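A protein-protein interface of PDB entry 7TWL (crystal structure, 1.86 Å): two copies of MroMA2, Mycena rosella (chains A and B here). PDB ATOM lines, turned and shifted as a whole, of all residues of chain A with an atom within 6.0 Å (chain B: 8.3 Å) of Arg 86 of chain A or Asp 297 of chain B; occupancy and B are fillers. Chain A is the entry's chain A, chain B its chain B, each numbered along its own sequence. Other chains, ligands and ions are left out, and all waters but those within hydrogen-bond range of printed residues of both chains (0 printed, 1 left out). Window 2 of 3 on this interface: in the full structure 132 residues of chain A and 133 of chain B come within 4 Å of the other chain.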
ATOM      1  N   SER A  81     -22.153 -13.691  13.498  1.00  0.00           N
ATOM      2  CA  SER A  81     -23.158 -13.666  14.553  1.00  0.00           C
ATOM      3  C   SER A  81     -22.492 -13.447  15.911  1.00  0.00           C
ATOM      4  O   SER A  81     -23.038 -12.745  16.755  1.00  0.00           O
ATOM      5  CB  SER A  81     -23.965 -14.948  14.593  1.00  0.00           C
ATOM      6  OG  SER A  81     -24.792 -15.074  13.441  1.00  0.00           O
ATOM      7  N   GLU A  82     -21.342 -14.106  16.131  1.00  0.00           N
ATOM      8  CA  GLU A  82     -20.760 -14.190  17.468  1.00  0.00           C
ATOM      9  C   GLU A  82     -20.212 -12.838  17.927  1.00  0.00           C
ATOM     10  O   GLU A  82     -20.396 -12.469  19.087  1.00  0.00           O
ATOM     11  CB  GLU A  82     -19.680 -15.280  17.540  1.00  0.00           C
ATOM     12  CG  GLU A  82     -19.380 -15.701  18.981  1.00  0.00           C
ATOM     13  CD  GLU A  82     -20.545 -16.364  19.713  1.00  0.00           C
ATOM     14  OE1 GLU A  82     -21.531 -16.761  19.044  1.00  0.00           O
ATOM     15  OE2 GLU A  82     -20.464 -16.500  20.959  1.00  0.00           O
ATOM     16  N   VAL A  83     -19.540 -12.098  17.031  1.00  0.00           N
ATOM     17  CA  VAL A  83     -18.961 -10.809  17.415  1.00  0.00           C
ATOM     18  C   VAL A  83     -20.069  -9.837  17.815  1.00  0.00           C
ATOM     19  O   VAL A  83     -19.870  -9.031  18.722  1.00  0.00           O
ATOM     20  CB  VAL A  83     -18.002 -10.184  16.376  1.00  0.00           C
ATOM     21  CG1 VAL A  83     -16.678 -10.938  16.269  1.00  0.00           C
ATOM     22  CG2 VAL A  83     -18.633  -9.976  15.000  1.00  0.00           C
ATOM     23  N   MET A  84     -21.232  -9.905  17.129  1.00  0.00           N
ATOM     24  CA  MET A  84     -22.378  -9.089  17.516  1.00  0.00           C
ATOM     25  C   MET A  84     -22.873  -9.485  18.917  1.00  0.00           C
ATOM     26  O   MET A  84     -23.093  -8.622  19.769  1.00  0.00           O
ATOM     27  CB  MET A  84     -23.527  -9.206  16.499  1.00  0.00           C
ATOM     28  CG  MET A  84     -23.225  -8.544  15.148  1.00  0.00           C
ATOM     29  SD  MET A  84     -24.618  -8.488  13.948  1.00  0.00           S
ATOM     30  CE  MET A  84     -24.733 -10.218  13.485  1.00  0.00           C
ATOM     31  N   LEU A  85     -23.021 -10.789  19.171  1.00  0.00           N
ATOM     32  CA  LEU A  85     -23.578 -11.264  20.435  1.00  0.00           C
ATOM     33  C   LEU A  85     -22.675 -10.910  21.622  1.00  0.00           C
ATOM     34  O   LEU A  85     -23.169 -10.677  22.720  1.00  0.00           O
ATOM     35  CB  LEU A  85     -23.815 -12.775  20.361  1.00  0.00           C
ATOM     36  CG  LEU A  85     -24.963 -13.237  19.455  1.00  0.00           C
ATOM     37  CD1 LEU A  85     -24.815 -14.721  19.122  1.00  0.00           C
ATOM     38  CD2 LEU A  85     -26.314 -12.948  20.095  1.00  0.00           C
ATOM     39  N   ARG A  86     -21.355 -10.868  21.396  1.00  0.00           N
ATOM     40  CA  ARG A  86     -20.388 -10.537  22.439  1.00  0.00           C
ATOM     41  C   ARG A  86     -20.601  -9.116  22.948  1.00  0.00           C
ATOM     42  O   ARG A  86     -20.510  -8.857  24.146  1.00  0.00           O
ATOM     43  CB  ARG A  86     -18.962 -10.655  21.895  1.00  0.00           C
ATOM     44  CG  ARG A  86     -18.444 -12.083  21.849  1.00  0.00           C
ATOM     45  CD  ARG A  86     -17.009 -12.122  21.350  1.00  0.00           C
ATOM     46  NE  ARG A  86     -16.523 -13.495  21.273  1.00  0.00           N
ATOM     47  CZ  ARG A  86     -15.285 -13.841  20.932  1.00  0.00           C
ATOM     48  NH1 ARG A  86     -14.395 -12.913  20.627  1.00  0.00           N
ATOM     49  NH2 ARG A  86     -14.941 -15.118  20.900  1.00  0.00           N
ATOM     50  N   ASP A  87     -20.880  -8.190  22.026  1.00  0.00           N
ATOM     51  CA  ASP A  87     -21.089  -6.801  22.394  1.00  0.00           C
ATOM     52  C   ASP A  87     -22.462  -6.613  23.040  1.00  0.00           C
ATOM     53  O   ASP A  87     -22.624  -5.743  23.899  1.00  0.00           O
ATOM     54  CB  ASP A  87     -20.829  -5.858  21.217  1.00  0.00           C
ATOM     55  CG  ASP A  87     -19.374  -5.437  21.126  1.00  0.00           C
ATOM     56  OD1 ASP A  87     -18.795  -5.125  22.182  1.00  0.00           O
ATOM     57  OD2 ASP A  87     -18.825  -5.455  20.017  1.00  0.00           O
ATOM     58  N   VAL A  88     -23.444  -7.410  22.602  1.00  0.00           N
ATOM     59  CA  VAL A  88     -24.748  -7.439  23.248  1.00  0.00           C
ATOM     60  C   VAL A  88     -24.569  -7.897  24.698  1.00  0.00           C
ATOM     61  O   VAL A  88     -25.128  -7.296  25.612  1.00  0.00           O
ATOM     62  CB  VAL A  88     -25.750  -8.330  22.489  1.00  0.00           C
ATOM     63  CG1 VAL A  88     -27.063  -8.468  23.249  1.00  0.00           C
ATOM     64  CG2 VAL A  88     -26.018  -7.791  21.087  1.00  0.00           C
ATOM     65  N   ARG A  89     -23.787  -8.970  24.882  1.00  0.00           N
ATOM     66  CA  ARG A  89     -23.521  -9.519  26.203  1.00  0.00           C
ATOM     67  C   ARG A  89     -22.812  -8.462  27.055  1.00  0.00           C
ATOM     68  O   ARG A  89     -23.011  -8.417  28.264  1.00  0.00           O
ATOM     69  CB  ARG A  89     -22.762 -10.849  26.098  1.00  0.00           C
ATOM     70  CG  ARG A  89     -23.612 -12.017  25.605  1.00  0.00           C
ATOM     71  CD  ARG A  89     -22.795 -13.196  25.109  1.00  0.00           C
ATOM     72  NE  ARG A  89     -23.571 -14.246  24.445  1.00  0.00           N
ATOM     73  CZ  ARG A  89     -23.127 -15.011  23.445  1.00  0.00           C
ATOM     74  NH1 ARG A  89     -21.903 -14.854  22.967  1.00  0.00           N
ATOM     75  NH2 ARG A  89     -23.907 -15.936  22.925  1.00  0.00           N
ATOM     76  N   ALA A  90     -22.022  -7.593  26.414  1.00  0.00           N
ATOM     77  CA  ALA A  90     -21.300  -6.536  27.107  1.00  0.00           C
ATOM     78  C   ALA A  90     -22.229  -5.378  27.465  1.00  0.00           C
ATOM     79  O   ALA A  90     -21.796  -4.422  28.102  1.00  0.00           O
ATOM     80  CB  ALA A  90     -20.128  -6.066  26.278  1.00  0.00           C
ATOM     81  N   GLY A  91     -23.498  -5.461  27.040  1.00  0.00           N
ATOM     82  CA  GLY A  91     -24.505  -4.498  27.444  1.00  0.00           C
ATOM     83  C   GLY A  91     -24.541  -3.263  26.544  1.00  0.00           C
ATOM     84  O   GLY A  91     -25.076  -2.228  26.943  1.00  0.00           O
ATOM     85  N   TYR B 285     -25.500 -23.982  19.432  1.00  0.00           N
ATOM     86  CA  TYR B 285     -24.064 -24.138  19.599  1.00  0.00           C
ATOM     87  C   TYR B 285     -23.696 -25.619  19.566  1.00  0.00           C
ATOM     88  O   TYR B 285     -23.196 -26.160  20.553  1.00  0.00           O
ATOM     89  CB  TYR B 285     -23.584 -23.409  20.858  1.00  0.00           C
ATOM     90  CG  TYR B 285     -23.588 -21.900  20.771  1.00  0.00           C
ATOM     91  CD1 TYR B 285     -22.567 -21.219  20.122  1.00  0.00           C
ATOM     92  CD2 TYR B 285     -24.590 -21.151  21.372  1.00  0.00           C
ATOM     93  CE1 TYR B 285     -22.558 -19.834  20.042  1.00  0.00           C
ATOM     94  CE2 TYR B 285     -24.588 -19.765  21.319  1.00  0.00           C
ATOM     95  CZ  TYR B 285     -23.575 -19.104  20.639  1.00  0.00           C
ATOM     96  OH  TYR B 285     -23.557 -17.736  20.576  1.00  0.00           O
ATOM     97  N   ARG B 291     -16.701 -24.801  17.277  1.00  0.00           N
ATOM     98  CA  ARG B 291     -15.365 -24.769  16.702  1.00  0.00           C
ATOM     99  C   ARG B 291     -15.121 -23.419  16.019  1.00  0.00           C
ATOM    100  O   ARG B 291     -14.043 -22.832  16.146  1.00  0.00           O
ATOM    101  CB  ARG B 291     -15.228 -25.913  15.695  1.00  0.00           C
ATOM    102  CG  ARG B 291     -13.805 -26.400  15.468  1.00  0.00           C
ATOM    103  CD  ARG B 291     -13.809 -27.738  14.749  1.00  0.00           C
ATOM    104  NE  ARG B 291     -14.647 -27.680  13.559  1.00  0.00           N
ATOM    105  CZ  ARG B 291     -15.776 -28.368  13.383  1.00  0.00           C
ATOM    106  NH1 ARG B 291     -16.204 -29.209  14.313  1.00  0.00           N
ATOM    107  NH2 ARG B 291     -16.463 -28.224  12.266  1.00  0.00           N
ATOM    108  N   ALA B 292     -16.131 -22.937  15.276  1.00  0.00           N
ATOM    109  CA  ALA B 292     -16.008 -21.660  14.587  1.00  0.00           C
ATOM    110  C   ALA B 292     -15.808 -20.533  15.597  1.00  0.00           C
ATOM    111  O   ALA B 292     -14.988 -19.645  15.370  1.00  0.00           O
ATOM    112  CB  ALA B 292     -17.199 -21.413  13.686  1.00  0.00           C
ATOM    113  N   VAL B 293     -16.533 -20.587  16.723  1.00  0.00           N
ATOM    114  CA  VAL B 293     -16.448 -19.529  17.715  1.00  0.00           C
ATOM    115  C   VAL B 293     -15.062 -19.547  18.356  1.00  0.00           C
ATOM    116  O   VAL B 293     -14.486 -18.491  18.592  1.00  0.00           O
ATOM    117  CB  VAL B 293     -17.585 -19.586  18.754  1.00  0.00           C
ATOM    118  CG1 VAL B 293     -17.283 -18.720  19.970  1.00  0.00           C
ATOM    119  CG2 VAL B 293     -18.939 -19.200  18.147  1.00  0.00           C
ATOM    120  N   ALA B 294     -14.523 -20.749  18.604  1.00  0.00           N
ATOM    121  CA  ALA B 294     -13.225 -20.889  19.246  1.00  0.00           C
ATOM    122  C   ALA B 294     -12.118 -20.355  18.334  1.00  0.00           C
ATOM    123  O   ALA B 294     -11.157 -19.765  18.816  1.00  0.00           O
ATOM    124  CB  ALA B 294     -13.002 -22.339  19.624  1.00  0.00           C
ATOM    125  N   ALA B 295     -12.279 -20.514  17.011  1.00  0.00           N
ATOM    126  CA  ALA B 295     -11.270 -20.110  16.036  1.00  0.00           C
ATOM    127  C   ALA B 295     -11.272 -18.596  15.770  1.00  0.00           C
ATOM    128  O   ALA B 295     -10.324 -18.057  15.208  1.00  0.00           O
ATOM    129  CB  ALA B 295     -11.454 -20.896  14.753  1.00  0.00           C
ATOM    130  N   LEU B 296     -12.340 -17.908  16.179  1.00  0.00           N
ATOM    131  CA  LEU B 296     -12.611 -16.516  15.832  1.00  0.00           C
ATOM    132  C   LEU B 296     -11.431 -15.586  16.157  1.00  0.00           C
ATOM    133  O   LEU B 296     -10.966 -14.847  15.292  1.00  0.00           O
ATOM    134  CB  LEU B 296     -13.870 -16.146  16.621  1.00  0.00           C
ATOM    135  CG  LEU B 296     -14.628 -14.870  16.270  1.00  0.00           C
ATOM    136  CD1 LEU B 296     -15.942 -14.870  17.040  1.00  0.00           C
ATOM    137  CD2 LEU B 296     -13.818 -13.638  16.667  1.00  0.00           C
ATOM    138  N   ASP B 297     -10.949 -15.607  17.404  1.00  0.00           N
ATOM    139  CA  ASP B 297     -10.023 -14.587  17.886  1.00  0.00           C
ATOM    140  C   ASP B 297      -8.671 -14.663  17.177  1.00  0.00           C
ATOM    141  O   ASP B 297      -7.998 -13.644  17.009  1.00  0.00           O
ATOM    142  CB  ASP B 297      -9.845 -14.646  19.404  1.00  0.00           C
ATOM    143  CG  ASP B 297     -11.104 -14.260  20.158  1.00  0.00           C
ATOM    144  OD1 ASP B 297     -11.527 -15.042  21.031  1.00  0.00           O
ATOM    145  OD2 ASP B 297     -11.637 -13.172  19.884  1.00  0.00           O
ATOM    146  N   SER B 298      -8.270 -15.865  16.762  1.00  0.00           N
ATOM    147  CA  SER B 298      -6.945 -16.026  16.186  1.00  0.00           C
ATOM    148  C   SER B 298      -7.003 -16.076  14.658  1.00  0.00           C
ATOM    149  O   SER B 298      -5.967 -16.258  14.008  1.00  0.00           O
ATOM    150  CB  SER B 298      -6.263 -17.240  16.763  1.00  0.00           C
ATOM    151  OG  SER B 298      -6.954 -18.417  16.377  1.00  0.00           O
ATOM    152  N   PHE B 299      -8.208 -15.906  14.085  1.00  0.00           N
ATOM    153  CA  PHE B 299      -8.350 -15.940  12.636  1.00  0.00           C
ATOM    154  C   PHE B 299      -7.530 -14.823  11.999  1.00  0.00           C
ATOM    155  O   PHE B 299      -7.661 -13.655  12.363  1.00  0.00           O
ATOM    156  CB  PHE B 299      -9.808 -15.843  12.164  1.00  0.00           C
ATOM    157  CG  PHE B 299      -9.953 -15.665  10.672  1.00  0.00           C
ATOM    158  CD1 PHE B 299      -9.623 -16.692   9.795  1.00  0.00           C
ATOM    159  CD2 PHE B 299     -10.425 -14.468  10.141  1.00  0.00           C
ATOM    160  CE1 PHE B 299      -9.734 -16.525   8.422  1.00  0.00           C
ATOM    161  CE2 PHE B 299     -10.549 -14.303   8.770  1.00  0.00           C
ATOM    162  CZ  PHE B 299     -10.205 -15.329   7.912  1.00  0.00           C
ATOM    163  N   VAL B 300      -6.706 -15.216  11.027  1.00  0.00           N
ATOM    164  CA  VAL B 300      -5.936 -14.289  10.215  1.00  0.00           C
ATOM    165  C   VAL B 300      -6.157 -14.660   8.750  1.00  0.00           C
ATOM    166  O   VAL B 300      -5.985 -15.815   8.365  1.00  0.00           O
ATOM    167  CB  VAL B 300      -4.441 -14.291  10.606  1.00  0.00           C
ATOM    168  CG1 VAL B 300      -3.836 -15.686  10.585  1.00  0.00           C
ATOM    169  CG2 VAL B 300      -3.616 -13.328   9.763  1.00  0.00           C
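Of the printed residues of chain B, Val 83 of chain A touches Leu 296 (3.95 Å).
Of the printed residues of chain B, Leu 85 of chain A touches Tyr 285 (3.6 Å).
Of the printed residues of chain B, Arg 86 of chain A touches Leu 296 and Asp 297.
Of the printed residues of chain B, Arg 89 of chain A touches Tyr 285 (3.0 Å).
Printed residues of chain A within 4 Å of Tyr 285 of chain B: Glu 82, Leu 85 and Arg 89.
Asp 297 of chain B touches just one residue of chain A: Arg 86.
OH of Tyr 285 of chain B sits at hydrogen-bond distance from OE1 of Glu 82 of chain A (2.7 Å).
NH1 of Arg 86 of chain A lies within salt-bridge range of OD2 of Asp 297 of chain B.
The side-chain hydroxyl of Tyr 285 of chain B sits at hydrogen-bond distance from the guanidinium group of Arg 89 of chain A.
The side-chain carboxylate of Glu 82 of chain A lies within salt-bridge range of the guanidinium group of Arg 89 of chain A (3.0 Å).
Glu 82 of chain A touches Val 293 of chain B.
CD1 of Leu 296 of chain B touches CB of Glu 82 of chain A, at 3.8 Å.
Leu 296 of chain B touches Val 83 of chain A.
OH of Tyr 285 of chain B touches CD1 of Leu 85 of chain A, at 3.6 Å.
NH2 of Arg 86 of chain A touches CD1 of Leu 296 of chain B, 3.995 Å away.
No position is printed for both chains.
Of the 8 pairs that touch across the chains among the printed residues, none has its exchanged pair printed and touching as well.
Printed residues of chain B that touch a printed residue of chain A: Tyr 285, Val 293, Leu 296 and Asp 297.
Hydrophobic or aromatic side chains of chain A within 4 Å of the printed part of chain B: Val 83 and Leu 85.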
